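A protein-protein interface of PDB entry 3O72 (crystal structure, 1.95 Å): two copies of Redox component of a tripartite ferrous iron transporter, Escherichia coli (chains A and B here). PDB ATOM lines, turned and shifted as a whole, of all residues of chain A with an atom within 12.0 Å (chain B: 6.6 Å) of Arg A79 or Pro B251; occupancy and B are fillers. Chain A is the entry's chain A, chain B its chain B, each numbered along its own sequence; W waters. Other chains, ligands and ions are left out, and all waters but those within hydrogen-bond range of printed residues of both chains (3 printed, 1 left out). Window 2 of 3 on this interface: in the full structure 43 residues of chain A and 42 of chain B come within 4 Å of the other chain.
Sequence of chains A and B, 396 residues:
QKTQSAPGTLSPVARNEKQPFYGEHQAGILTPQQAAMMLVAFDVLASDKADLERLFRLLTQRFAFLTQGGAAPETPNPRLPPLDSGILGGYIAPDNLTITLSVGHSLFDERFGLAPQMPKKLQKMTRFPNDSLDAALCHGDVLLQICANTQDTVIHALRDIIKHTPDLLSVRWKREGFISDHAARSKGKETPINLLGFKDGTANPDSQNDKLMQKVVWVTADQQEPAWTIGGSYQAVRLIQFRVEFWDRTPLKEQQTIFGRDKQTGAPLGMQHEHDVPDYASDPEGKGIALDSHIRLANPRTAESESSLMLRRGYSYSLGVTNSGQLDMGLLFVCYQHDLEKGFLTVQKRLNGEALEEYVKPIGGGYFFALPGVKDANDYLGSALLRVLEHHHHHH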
ATOM      1  N   GLU A  74     -16.255 -34.125  28.174  1.00  0.00           N
ATOM      2  CA  GLU A  74     -16.275 -33.443  26.877  1.00  0.00           C
ATOM      3  C   GLU A  74     -17.695 -33.258  26.330  1.00  0.00           C
ATOM      4  O   GLU A  74     -18.644 -33.863  26.821  1.00  0.00           O
ATOM      5  CB  GLU A  74     -15.428 -34.194  25.852  1.00  0.00           C
ATOM      6  CG  GLU A  74     -13.943 -33.833  25.860  1.00  0.00           C
ATOM      7  CD  GLU A  74     -13.214 -34.392  24.652  1.00  0.00           C
ATOM      8  OE1 GLU A  74     -13.629 -35.470  24.154  1.00  0.00           O
ATOM      9  OE2 GLU A  74     -12.237 -33.749  24.199  1.00  0.00           O
ATOM     10  N   THR A  75     -17.826 -32.425  25.302  1.00  0.00           N
ATOM     11  CA  THR A  75     -19.137 -32.090  24.728  1.00  0.00           C
ATOM     12  C   THR A  75     -19.159 -32.369  23.220  1.00  0.00           C
ATOM     13  O   THR A  75     -19.112 -31.444  22.409  1.00  0.00           O
ATOM     14  CB  THR A  75     -19.517 -30.596  25.009  1.00  0.00           C
ATOM     15  OG1 THR A  75     -19.478 -30.347  26.426  1.00  0.00           O
ATOM     16  CG2 THR A  75     -20.912 -30.274  24.474  1.00  0.00           C
ATOM     17  N   PRO A  76     -19.235 -33.655  22.845  1.00  0.00           N
ATOM     18  CA  PRO A  76     -19.146 -34.110  21.446  1.00  0.00           C
ATOM     19  C   PRO A  76     -20.200 -33.465  20.557  1.00  0.00           C
ATOM     20  O   PRO A  76     -19.947 -33.157  19.392  1.00  0.00           O
ATOM     21  CB  PRO A  76     -19.414 -35.611  21.552  1.00  0.00           C
ATOM     22  CG  PRO A  76     -19.066 -35.960  22.957  1.00  0.00           C
ATOM     23  CD  PRO A  76     -19.449 -34.775  23.778  1.00  0.00           C
ATOM     24  N   ASN A  77     -21.383 -33.275  21.122  1.00  0.00           N
ATOM     25  CA  ASN A  77     -22.469 -32.592  20.440  1.00  0.00           C
ATOM     26  C   ASN A  77     -22.652 -31.165  20.976  1.00  0.00           C
ATOM     27  O   ASN A  77     -23.182 -30.973  22.068  1.00  0.00           O
ATOM     28  CB  ASN A  77     -23.766 -33.377  20.608  1.00  0.00           C
ATOM     29  CG  ASN A  77     -24.940 -32.678  19.982  1.00  0.00           C
ATOM     30  OD1 ASN A  77     -24.768 -31.692  19.267  1.00  0.00           O
ATOM     31  ND2 ASN A  77     -26.145 -33.183  20.235  1.00  0.00           N
ATOM     32  N   PRO A  78     -22.216 -30.163  20.199  1.00  0.00           N
ATOM     33  CA  PRO A  78     -22.250 -28.762  20.646  1.00  0.00           C
ATOM     34  C   PRO A  78     -23.657 -28.164  20.691  1.00  0.00           C
ATOM     35  O   PRO A  78     -23.807 -27.036  21.159  1.00  0.00           O
ATOM     36  CB  PRO A  78     -21.386 -28.028  19.609  1.00  0.00           C
ATOM     37  CG  PRO A  78     -20.703 -29.118  18.801  1.00  0.00           C
ATOM     38  CD  PRO A  78     -21.604 -30.305  18.869  1.00  0.00           C
ATOM     39  N   ARG A  79     -24.669 -28.890  20.225  1.00  0.00           N
ATOM     40  CA  ARG A  79     -26.047 -28.417  20.365  1.00  0.00           C
ATOM     41  C   ARG A  79     -26.535 -28.588  21.812  1.00  0.00           C
ATOM     42  O   ARG A  79     -27.579 -28.071  22.200  1.00  0.00           O
ATOM     43  CB  ARG A  79     -26.971 -29.109  19.359  1.00  0.00           C
ATOM     44  CG  ARG A  79     -26.605 -28.783  17.904  1.00  0.00           C
ATOM     45  CD  ARG A  79     -27.529 -29.455  16.876  1.00  0.00           C
ATOM     46  NE  ARG A  79     -27.522 -30.916  16.962  1.00  0.00           N
ATOM     47  CZ  ARG A  79     -26.490 -31.696  16.630  1.00  0.00           C
ATOM     48  NH1 ARG A  79     -25.347 -31.166  16.200  1.00  0.00           N
ATOM     49  NH2 ARG A  79     -26.597 -33.016  16.738  1.00  0.00           N
ATOM     50  N   LEU A  80     -25.756 -29.301  22.606  1.00  0.00           N
ATOM     51  CA  LEU A  80     -26.037 -29.457  24.029  1.00  0.00           C
ATOM     52  C   LEU A  80     -25.194 -28.493  24.856  1.00  0.00           C
ATOM     53  O   LEU A  80     -24.096 -28.091  24.435  1.00  0.00           O
ATOM     54  CB  LEU A  80     -25.734 -30.890  24.485  1.00  0.00           C
ATOM     55  CG  LEU A  80     -26.503 -32.043  23.832  1.00  0.00           C
ATOM     56  CD1 LEU A  80     -26.038 -33.364  24.418  1.00  0.00           C
ATOM     57  CD2 LEU A  80     -28.010 -31.864  24.030  1.00  0.00           C
ATOM     58  N   PRO A  81     -25.699 -28.127  26.045  1.00  0.00           N
ATOM     59  CA  PRO A  81     -24.878 -27.358  26.984  1.00  0.00           C
ATOM     60  C   PRO A  81     -23.597 -28.134  27.285  1.00  0.00           C
ATOM     61  O   PRO A  81     -23.624 -29.367  27.294  1.00  0.00           O
ATOM     62  CB  PRO A  81     -25.769 -27.255  28.221  1.00  0.00           C
ATOM     63  CG  PRO A  81     -27.171 -27.373  27.687  1.00  0.00           C
ATOM     64  CD  PRO A  81     -27.070 -28.342  26.535  1.00  0.00           C
ATOM     65  N   PRO A  82     -22.479 -27.427  27.495  1.00  0.00           N
ATOM     66  CA  PRO A  82     -21.217 -28.097  27.812  1.00  0.00           C
ATOM     67  C   PRO A  82     -21.427 -28.990  29.028  1.00  0.00           C
ATOM     68  O   PRO A  82     -22.144 -28.593  29.958  1.00  0.00           O
ATOM     69  CB  PRO A  82     -20.285 -26.932  28.171  1.00  0.00           C
ATOM     70  CG  PRO A  82     -20.889 -25.743  27.533  1.00  0.00           C
ATOM     71  CD  PRO A  82     -22.363 -25.957  27.560  1.00  0.00           C
ATOM     72  N   LEU A  83     -20.837 -30.180  29.023  1.00  0.00           N
ATOM     73  CA  LEU A  83     -21.019 -31.103  30.145  1.00  0.00           C
ATOM     74  C   LEU A  83     -20.220 -30.672  31.377  1.00  0.00           C
ATOM     75  O   LEU A  83     -20.465 -31.151  32.479  1.00  0.00           O
ATOM     76  CB  LEU A  83     -20.649 -32.539  29.745  1.00  0.00           C
ATOM     77  CG  LEU A  83     -21.742 -33.306  29.002  1.00  0.00           C
ATOM     78  CD1 LEU A  83     -22.064 -32.646  27.665  1.00  0.00           C
ATOM     79  CD2 LEU A  83     -21.342 -34.767  28.808  1.00  0.00           C
ATOM     80  N   ASP A  84     -19.240 -29.798  31.165  1.00  0.00           N
ATOM     81  CA  ASP A  84     -18.455 -29.204  32.250  1.00  0.00           C
ATOM     82  C   ASP A  84     -18.443 -27.692  32.034  1.00  0.00           C
ATOM     83  O   ASP A  84     -18.467 -27.239  30.891  1.00  0.00           O
ATOM     84  CB  ASP A  84     -17.015 -29.712  32.222  1.00  0.00           C
ATOM     85  CG  ASP A  84     -16.175 -29.149  33.364  1.00  0.00           C
ATOM     86  OD1 ASP A  84     -16.401 -29.567  34.521  1.00  0.00           O
ATOM     87  OD2 ASP A  84     -15.291 -28.294  33.117  1.00  0.00           O
ATOM     88  N   SER A  85     -18.399 -26.925  33.120  1.00  0.00           N
ATOM     89  CA  SER A  85     -18.401 -25.455  33.054  1.00  0.00           C
ATOM     90  C   SER A  85     -17.189 -24.892  32.319  1.00  0.00           C
ATOM     91  O   SER A  85     -17.242 -23.792  31.751  1.00  0.00           O
ATOM     92  CB  SER A  85     -18.431 -24.860  34.471  1.00  0.00           C
ATOM     93  OG  SER A  85     -17.170 -25.029  35.106  1.00  0.00           O
ATOM     94  N   GLY A  86     -16.084 -25.624  32.367  1.00  0.00           N
ATOM     95  CA  GLY A  86     -14.870 -25.228  31.681  1.00  0.00           C
ATOM     96  C   GLY A  86     -13.931 -24.341  32.479  1.00  0.00           C
ATOM     97  O   GLY A  86     -12.850 -23.994  31.995  1.00  0.00           O
ATOM     98  N   ARG A 159     -20.560 -25.686  40.564  1.00  0.00           N
ATOM     99  CA  ARG A 159     -21.218 -25.565  39.264  1.00  0.00           C
ATOM    100  C   ARG A 159     -21.518 -26.957  38.703  1.00  0.00           C
ATOM    101  O   ARG A 159     -22.552 -27.177  38.062  1.00  0.00           O
ATOM    102  CB  ARG A 159     -20.361 -24.762  38.274  1.00  0.00           C
ATOM    103  CG  ARG A 159     -20.013 -23.337  38.729  1.00  0.00           C
ATOM    104  CD  ARG A 159     -20.984 -22.298  38.190  1.00  0.00           C
ATOM    105  NE  ARG A 159     -20.908 -22.175  36.731  1.00  0.00           N
ATOM    106  CZ  ARG A 159     -20.105 -21.338  36.075  1.00  0.00           C
ATOM    107  NH1 ARG A 159     -19.282 -20.526  36.740  1.00  0.00           N
ATOM    108  NH2 ARG A 159     -20.126 -21.310  34.744  1.00  0.00           N
ATOM    109  N   LYS A 163     -25.317 -28.145  37.839  1.00  0.00           N
ATOM    110  CA  LYS A 163     -25.654 -28.581  36.486  1.00  0.00           C
ATOM    111  C   LYS A 163     -26.332 -29.958  36.528  1.00  0.00           C
ATOM    112  O   LYS A 163     -27.250 -30.222  35.764  1.00  0.00           O
ATOM    113  CB  LYS A 163     -24.406 -28.610  35.597  1.00  0.00           C
ATOM    114  CG  LYS A 163     -24.717 -28.847  34.112  1.00  0.00           C
ATOM    115  CD  LYS A 163     -23.763 -29.844  33.500  1.00  0.00           C
ATOM    116  CE  LYS A 163     -24.408 -30.537  32.291  1.00  0.00           C
ATOM    117  NZ  LYS A 163     -25.242 -29.580  31.510  1.00  0.00           N
ATOM    118  N   TRP B 247     -26.443 -19.508  31.784  1.00  0.00           N
ATOM    119  CA  TRP B 247     -25.336 -19.731  30.856  1.00  0.00           C
ATOM    120  C   TRP B 247     -24.981 -21.205  30.779  1.00  0.00           C
ATOM    121  O   TRP B 247     -24.854 -21.755  29.687  1.00  0.00           O
ATOM    122  CB  TRP B 247     -24.102 -18.959  31.317  1.00  0.00           C
ATOM    123  CG  TRP B 247     -22.831 -19.160  30.498  1.00  0.00           C
ATOM    124  CD1 TRP B 247     -21.733 -19.884  30.860  1.00  0.00           C
ATOM    125  CD2 TRP B 247     -22.517 -18.569  29.223  1.00  0.00           C
ATOM    126  NE1 TRP B 247     -20.763 -19.794  29.887  1.00  0.00           N
ATOM    127  CE2 TRP B 247     -21.221 -19.003  28.870  1.00  0.00           C
ATOM    128  CE3 TRP B 247     -23.215 -17.733  28.340  1.00  0.00           C
ATOM    129  CZ2 TRP B 247     -20.602 -18.618  27.677  1.00  0.00           C
ATOM    130  CZ3 TRP B 247     -22.604 -17.353  27.151  1.00  0.00           C
ATOM    131  CH2 TRP B 247     -21.310 -17.792  26.833  1.00  0.00           C
ATOM    132  N   ASP B 248     -24.810 -21.847  31.934  1.00  0.00           N
ATOM    133  CA  ASP B 248     -24.427 -23.263  31.948  1.00  0.00           C
ATOM    134  C   ASP B 248     -25.434 -24.203  31.264  1.00  0.00           C
ATOM    135  O   ASP B 248     -25.086 -25.337  30.908  1.00  0.00           O
ATOM    136  CB  ASP B 248     -24.151 -23.754  33.371  1.00  0.00           C
ATOM    137  CG  ASP B 248     -22.785 -23.315  33.904  1.00  0.00           C
ATOM    138  OD1 ASP B 248     -21.964 -22.755  33.149  1.00  0.00           O
ATOM    139  OD2 ASP B 248     -22.545 -23.528  35.107  1.00  0.00           O
ATOM    140  N   ARG B 249     -26.680 -23.779  31.097  1.00  0.00           N
ATOM    141  CA  ARG B 249     -27.578 -24.625  30.313  1.00  0.00           C
ATOM    142  C   ARG B 249     -27.802 -24.105  28.902  1.00  0.00           C
ATOM    143  O   ARG B 249     -28.804 -24.398  28.262  1.00  0.00           O
ATOM    144  CB  ARG B 249     -28.884 -24.942  31.035  1.00  0.00           C
ATOM    145  CG  ARG B 249     -29.493 -23.846  31.812  1.00  0.00           C
ATOM    146  CD  ARG B 249     -30.611 -24.373  32.743  1.00  0.00           C
ATOM    147  NE  ARG B 249     -31.446 -23.242  33.123  1.00  0.00           N
ATOM    148  CZ  ARG B 249     -31.324 -22.557  34.254  1.00  0.00           C
ATOM    149  NH1 ARG B 249     -30.438 -22.922  35.169  1.00  0.00           N
ATOM    150  NH2 ARG B 249     -32.114 -21.514  34.480  1.00  0.00           N
ATOM    151  N   THR B 250     -26.838 -23.335  28.417  1.00  0.00           N
ATOM    152  CA  THR B 250     -26.904 -22.799  27.064  1.00  0.00           C
ATOM    153  C   THR B 250     -25.995 -23.635  26.199  1.00  0.00           C
ATOM    154  O   THR B 250     -24.879 -23.953  26.608  1.00  0.00           O
ATOM    155  CB  THR B 250     -26.480 -21.325  27.029  1.00  0.00           C
ATOM    156  OG1 THR B 250     -27.425 -20.539  27.775  1.00  0.00           O
ATOM    157  CG2 THR B 250     -26.412 -20.819  25.586  1.00  0.00           C
ATOM    158  N   PRO B 251     -26.475 -24.028  25.004  1.00  0.00           N
ATOM    159  CA  PRO B 251     -25.657 -24.901  24.157  1.00  0.00           C
ATOM    160  C   PRO B 251     -24.259 -24.341  23.894  1.00  0.00           C
ATOM    161  O   PRO B 251     -24.073 -23.127  23.773  1.00  0.00           O
ATOM    162  CB  PRO B 251     -26.472 -24.987  22.861  1.00  0.00           C
ATOM    163  CG  PRO B 251     -27.904 -24.863  23.338  1.00  0.00           C
ATOM    164  CD  PRO B 251     -27.842 -23.851  24.464  1.00  0.00           C
ATOM    165  N   LEU B 252     -23.276 -25.232  23.824  1.00  0.00           N
ATOM    166  CA  LEU B 252     -21.899 -24.822  23.611  1.00  0.00           C
ATOM    167  C   LEU B 252     -21.753 -24.059  22.300  1.00  0.00           C
ATOM    168  O   LEU B 252     -21.016 -23.077  22.223  1.00  0.00           O
ATOM    169  CB  LEU B 252     -20.971 -26.038  23.619  1.00  0.00           C
ATOM    170  CG  LEU B 252     -19.539 -25.797  23.155  1.00  0.00           C
ATOM    171  CD1 LEU B 252     -18.792 -24.856  24.133  1.00  0.00           C
ATOM    172  CD2 LEU B 252     -18.812 -27.129  23.001  1.00  0.00           C
ATOM    173  N   LYS B 253     -22.454 -24.519  21.268  1.00  0.00           N
ATOM    174  CA  LYS B 253     -22.435 -23.827  19.983  1.00  0.00           C
ATOM    175  C   LYS B 253     -22.832 -22.367  20.173  1.00  0.00           C
ATOM    176  O   LYS B 253     -22.248 -21.459  19.569  1.00  0.00           O
ATOM    177  CB  LYS B 253     -23.395 -24.500  19.001  1.00  0.00           C
ATOM    178  CG  LYS B 253     -23.503 -23.800  17.651  1.00  0.00           C
ATOM    179  CD  LYS B 253     -24.537 -24.503  16.763  1.00  0.00           C
ATOM    180  CE  LYS B 253     -24.756 -23.754  15.453  1.00  0.00           C
ATOM    181  NZ  LYS B 253     -25.778 -24.431  14.597  1.00  0.00           N
ATOM    182  N   GLU B 254     -23.824 -22.138  21.018  1.00  0.00           N
ATOM    183  CA  GLU B 254     -24.279 -20.776  21.255  1.00  0.00           C
ATOM    184  C   GLU B 254     -23.272 -19.971  22.066  1.00  0.00           C
ATOM    185  O   GLU B 254     -23.029 -18.807  21.776  1.00  0.00           O
ATOM    186  CB  GLU B 254     -25.629 -20.748  21.959  1.00  0.00           C
ATOM    187  CG  GLU B 254     -26.120 -19.342  22.103  1.00  0.00           C
ATOM    188  CD  GLU B 254     -26.291 -18.711  20.742  1.00  0.00           C
ATOM    189  OE1 GLU B 254     -25.902 -17.536  20.556  1.00  0.00           O
ATOM    190  OE2 GLU B 254     -26.782 -19.425  19.837  1.00  0.00           O
ATOM    191  N   GLN B 255     -22.698 -20.576  23.099  1.00  0.00           N
ATOM    192  CA  GLN B 255     -21.648 -19.898  23.864  1.00  0.00           C
ATOM    193  C   GLN B 255     -20.519 -19.429  22.938  1.00  0.00           C
ATOM    194  O   GLN B 255     -20.029 -18.301  23.054  1.00  0.00           O
ATOM    195  CB  GLN B 255     -21.077 -20.823  24.935  1.00  0.00           C
ATOM    196  CG  GLN B 255     -22.093 -21.322  25.970  1.00  0.00           C
ATOM    197  CD  GLN B 255     -21.405 -21.968  27.166  1.00  0.00           C
ATOM    198  OE1 GLN B 255     -20.176 -22.094  27.200  1.00  0.00           O
ATOM    199  NE2 GLN B 255     -22.195 -22.369  28.159  1.00  0.00           N
ATOM    200  N   GLN B 256     -20.102 -20.305  22.029  1.00  0.00           N
ATOM    201  CA  GLN B 256     -19.013 -19.977  21.109  1.00  0.00           C
ATOM    202  C   GLN B 256     -19.398 -18.885  20.091  1.00  0.00           C
ATOM    203  O   GLN B 256     -18.601 -18.012  19.789  1.00  0.00           O
ATOM    204  CB  GLN B 256     -18.463 -21.253  20.441  1.00  0.00           C
ATOM    205  CG  GLN B 256     -17.850 -22.204  21.507  1.00  0.00           C
ATOM    206  CD  GLN B 256     -17.110 -23.430  20.967  1.00  0.00           C
ATOM    207  OE1 GLN B 256     -16.240 -23.966  21.649  1.00  0.00           O
ATOM    208  NE2 GLN B 256     -17.463 -23.884  19.771  1.00  0.00           N
ATOM    209  N   TYR B 359     -26.715 -12.658  29.146  1.00  0.00           N
ATOM    210  CA  TYR B 359     -26.070 -13.425  30.207  1.00  0.00           C
ATOM    211  C   TYR B 359     -25.328 -12.570  31.231  1.00  0.00           C
ATOM    212  O   TYR B 359     -24.866 -13.093  32.237  1.00  0.00           O
ATOM    213  CB  TYR B 359     -25.136 -14.483  29.610  1.00  0.00           C
ATOM    214  CG  TYR B 359     -25.873 -15.410  28.692  1.00  0.00           C
ATOM    215  CD1 TYR B 359     -26.628 -16.462  29.206  1.00  0.00           C
ATOM    216  CD2 TYR B 359     -25.852 -15.226  27.320  1.00  0.00           C
ATOM    217  CE1 TYR B 359     -27.334 -17.296  28.384  1.00  0.00           C
ATOM    218  CE2 TYR B 359     -26.553 -16.076  26.476  1.00  0.00           C
ATOM    219  CZ  TYR B 359     -27.296 -17.101  27.021  1.00  0.00           C
ATOM    220  OH  TYR B 359     -27.998 -17.947  26.212  1.00  0.00           O
HETATM  221  O   HOH W   1     -19.424 -22.330  31.590  1.00  0.00           O
HETATM  222  O   HOH W   2     -22.513 -26.365  31.260  1.00  0.00           O
HETATM  223  O   HOH W   3     -24.120 -24.730  36.778  1.00  0.00           O
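The backbone carbonyl oxygen (O) of Trp B247 sits at hydrogen-bond distance from the side-chain amide nitrogen (NE2) of Gln B255 (3.1 Å). The backbone carbonyl oxygen of Thr B250 lies within hydrogen-bond range of the side-chain amide nitrogen of Gln B255, 3.5 Å away. OG1 of Thr B250 sits at hydrogen-bond distance from OH of Tyr B359 (3.1 Å). The side-chain amide oxygen of Asn A77 lies within hydrogen-bond range of the backbone NH of Arg A79, 3.0 Å away. The backbone carbonyl oxygen (O) of Trp B247 lies close to the side-chain hydroxyl (OG1) of Thr B250 (3.4 Å).
Water W3 lies within hydrogen-bond range of OD2 of Asp B248 (2.6 Å) and O of Arg A159 (3.2 Å). Water W2 lies within hydrogen-bond range of O of Pro A82 (2.6 Å) and O of Asp B248 (2.8 Å). Water W1 lies within hydrogen-bond range of O of Ser A85 (2.6 Å), OD1 of Asp B248 (3.0 Å), NE1 of Trp B247 (3.3 Å) and NH2 of Arg A159 (3.4 Å).
Pro A78 touches Pro B251. Pro B251 touches Arg A79 (CB to O, 3.3 Å). Pro B251 touches Leu A80. Asp B248 touches Pro A81. Arg B249 touches Pro A81 (O to CG, 3.4 Å). Pro A81 touches Thr B250 (CA to O, 3.4 Å). Pro A81 touches Pro B251 (N to CA, 3.7 Å). Pro A82 touches Thr B250 (CD to O, 3.4 Å). Pro A82 touches Leu B252. Pro A82 touches Gln B255.
Of chain B, only Pro B251 (3.3 Å) comes within 4 Å of Arg A79. Of the printed residues of chain B, Pro A81 touches Asp B248 (3.4 Å), Arg B249 (3.4 Å), Thr B250 (3.4 Å) and Pro B251 (3.7 Å). Of the printed residues of chain B, Arg A159 touches Asp B248 (2.7 Å). Thr B250 touches just these residues of chain A: Pro A81 and Pro A82. Of chain A, only Pro A78, Arg A79, Leu A80 and Pro A81 come within 4 Å of Pro B251. Of chain A, only Pro A78, Leu A80 and Pro A82 come within 4 Å of Leu B252. Gln B255 touches just one residue of chain A: Pro A82 (3.6 Å). Gln B256 touches none of the printed residues of chain A. The nearest residue of chain B that does not touch Arg A79 is Lys B253 (4.7 Å). The nearest residue of chain A that does not touch Pro B251 is Pro A82 (4.4 Å).
No position is printed for both chains.
N of Leu B252 sits at hydrogen-bond distance from O of Pro A78 (3.3 Å). O of Leu A80 is in hydrogen-bond range of N of Leu B252, 3.0 Å away. The side-chain carboxylate of Asp B248 is in salt-bridge range of the guanidinium group of Arg A159 (2.7 Å). N of Lys B253 is in hydrogen-bond range of O of Pro A78, 2.9 Å away.
Along chain B the printed residues that touch a printed residue of chain A span positions 248 to 255. Among the printed residues, 14 pairs touch across the chains. Among the printed residues, Asp or Glu carboxylates within 4 Å of a Lys or Arg side-chain nitrogen of the other chain: Arg A159 with Asp B248 (2.7 Å).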
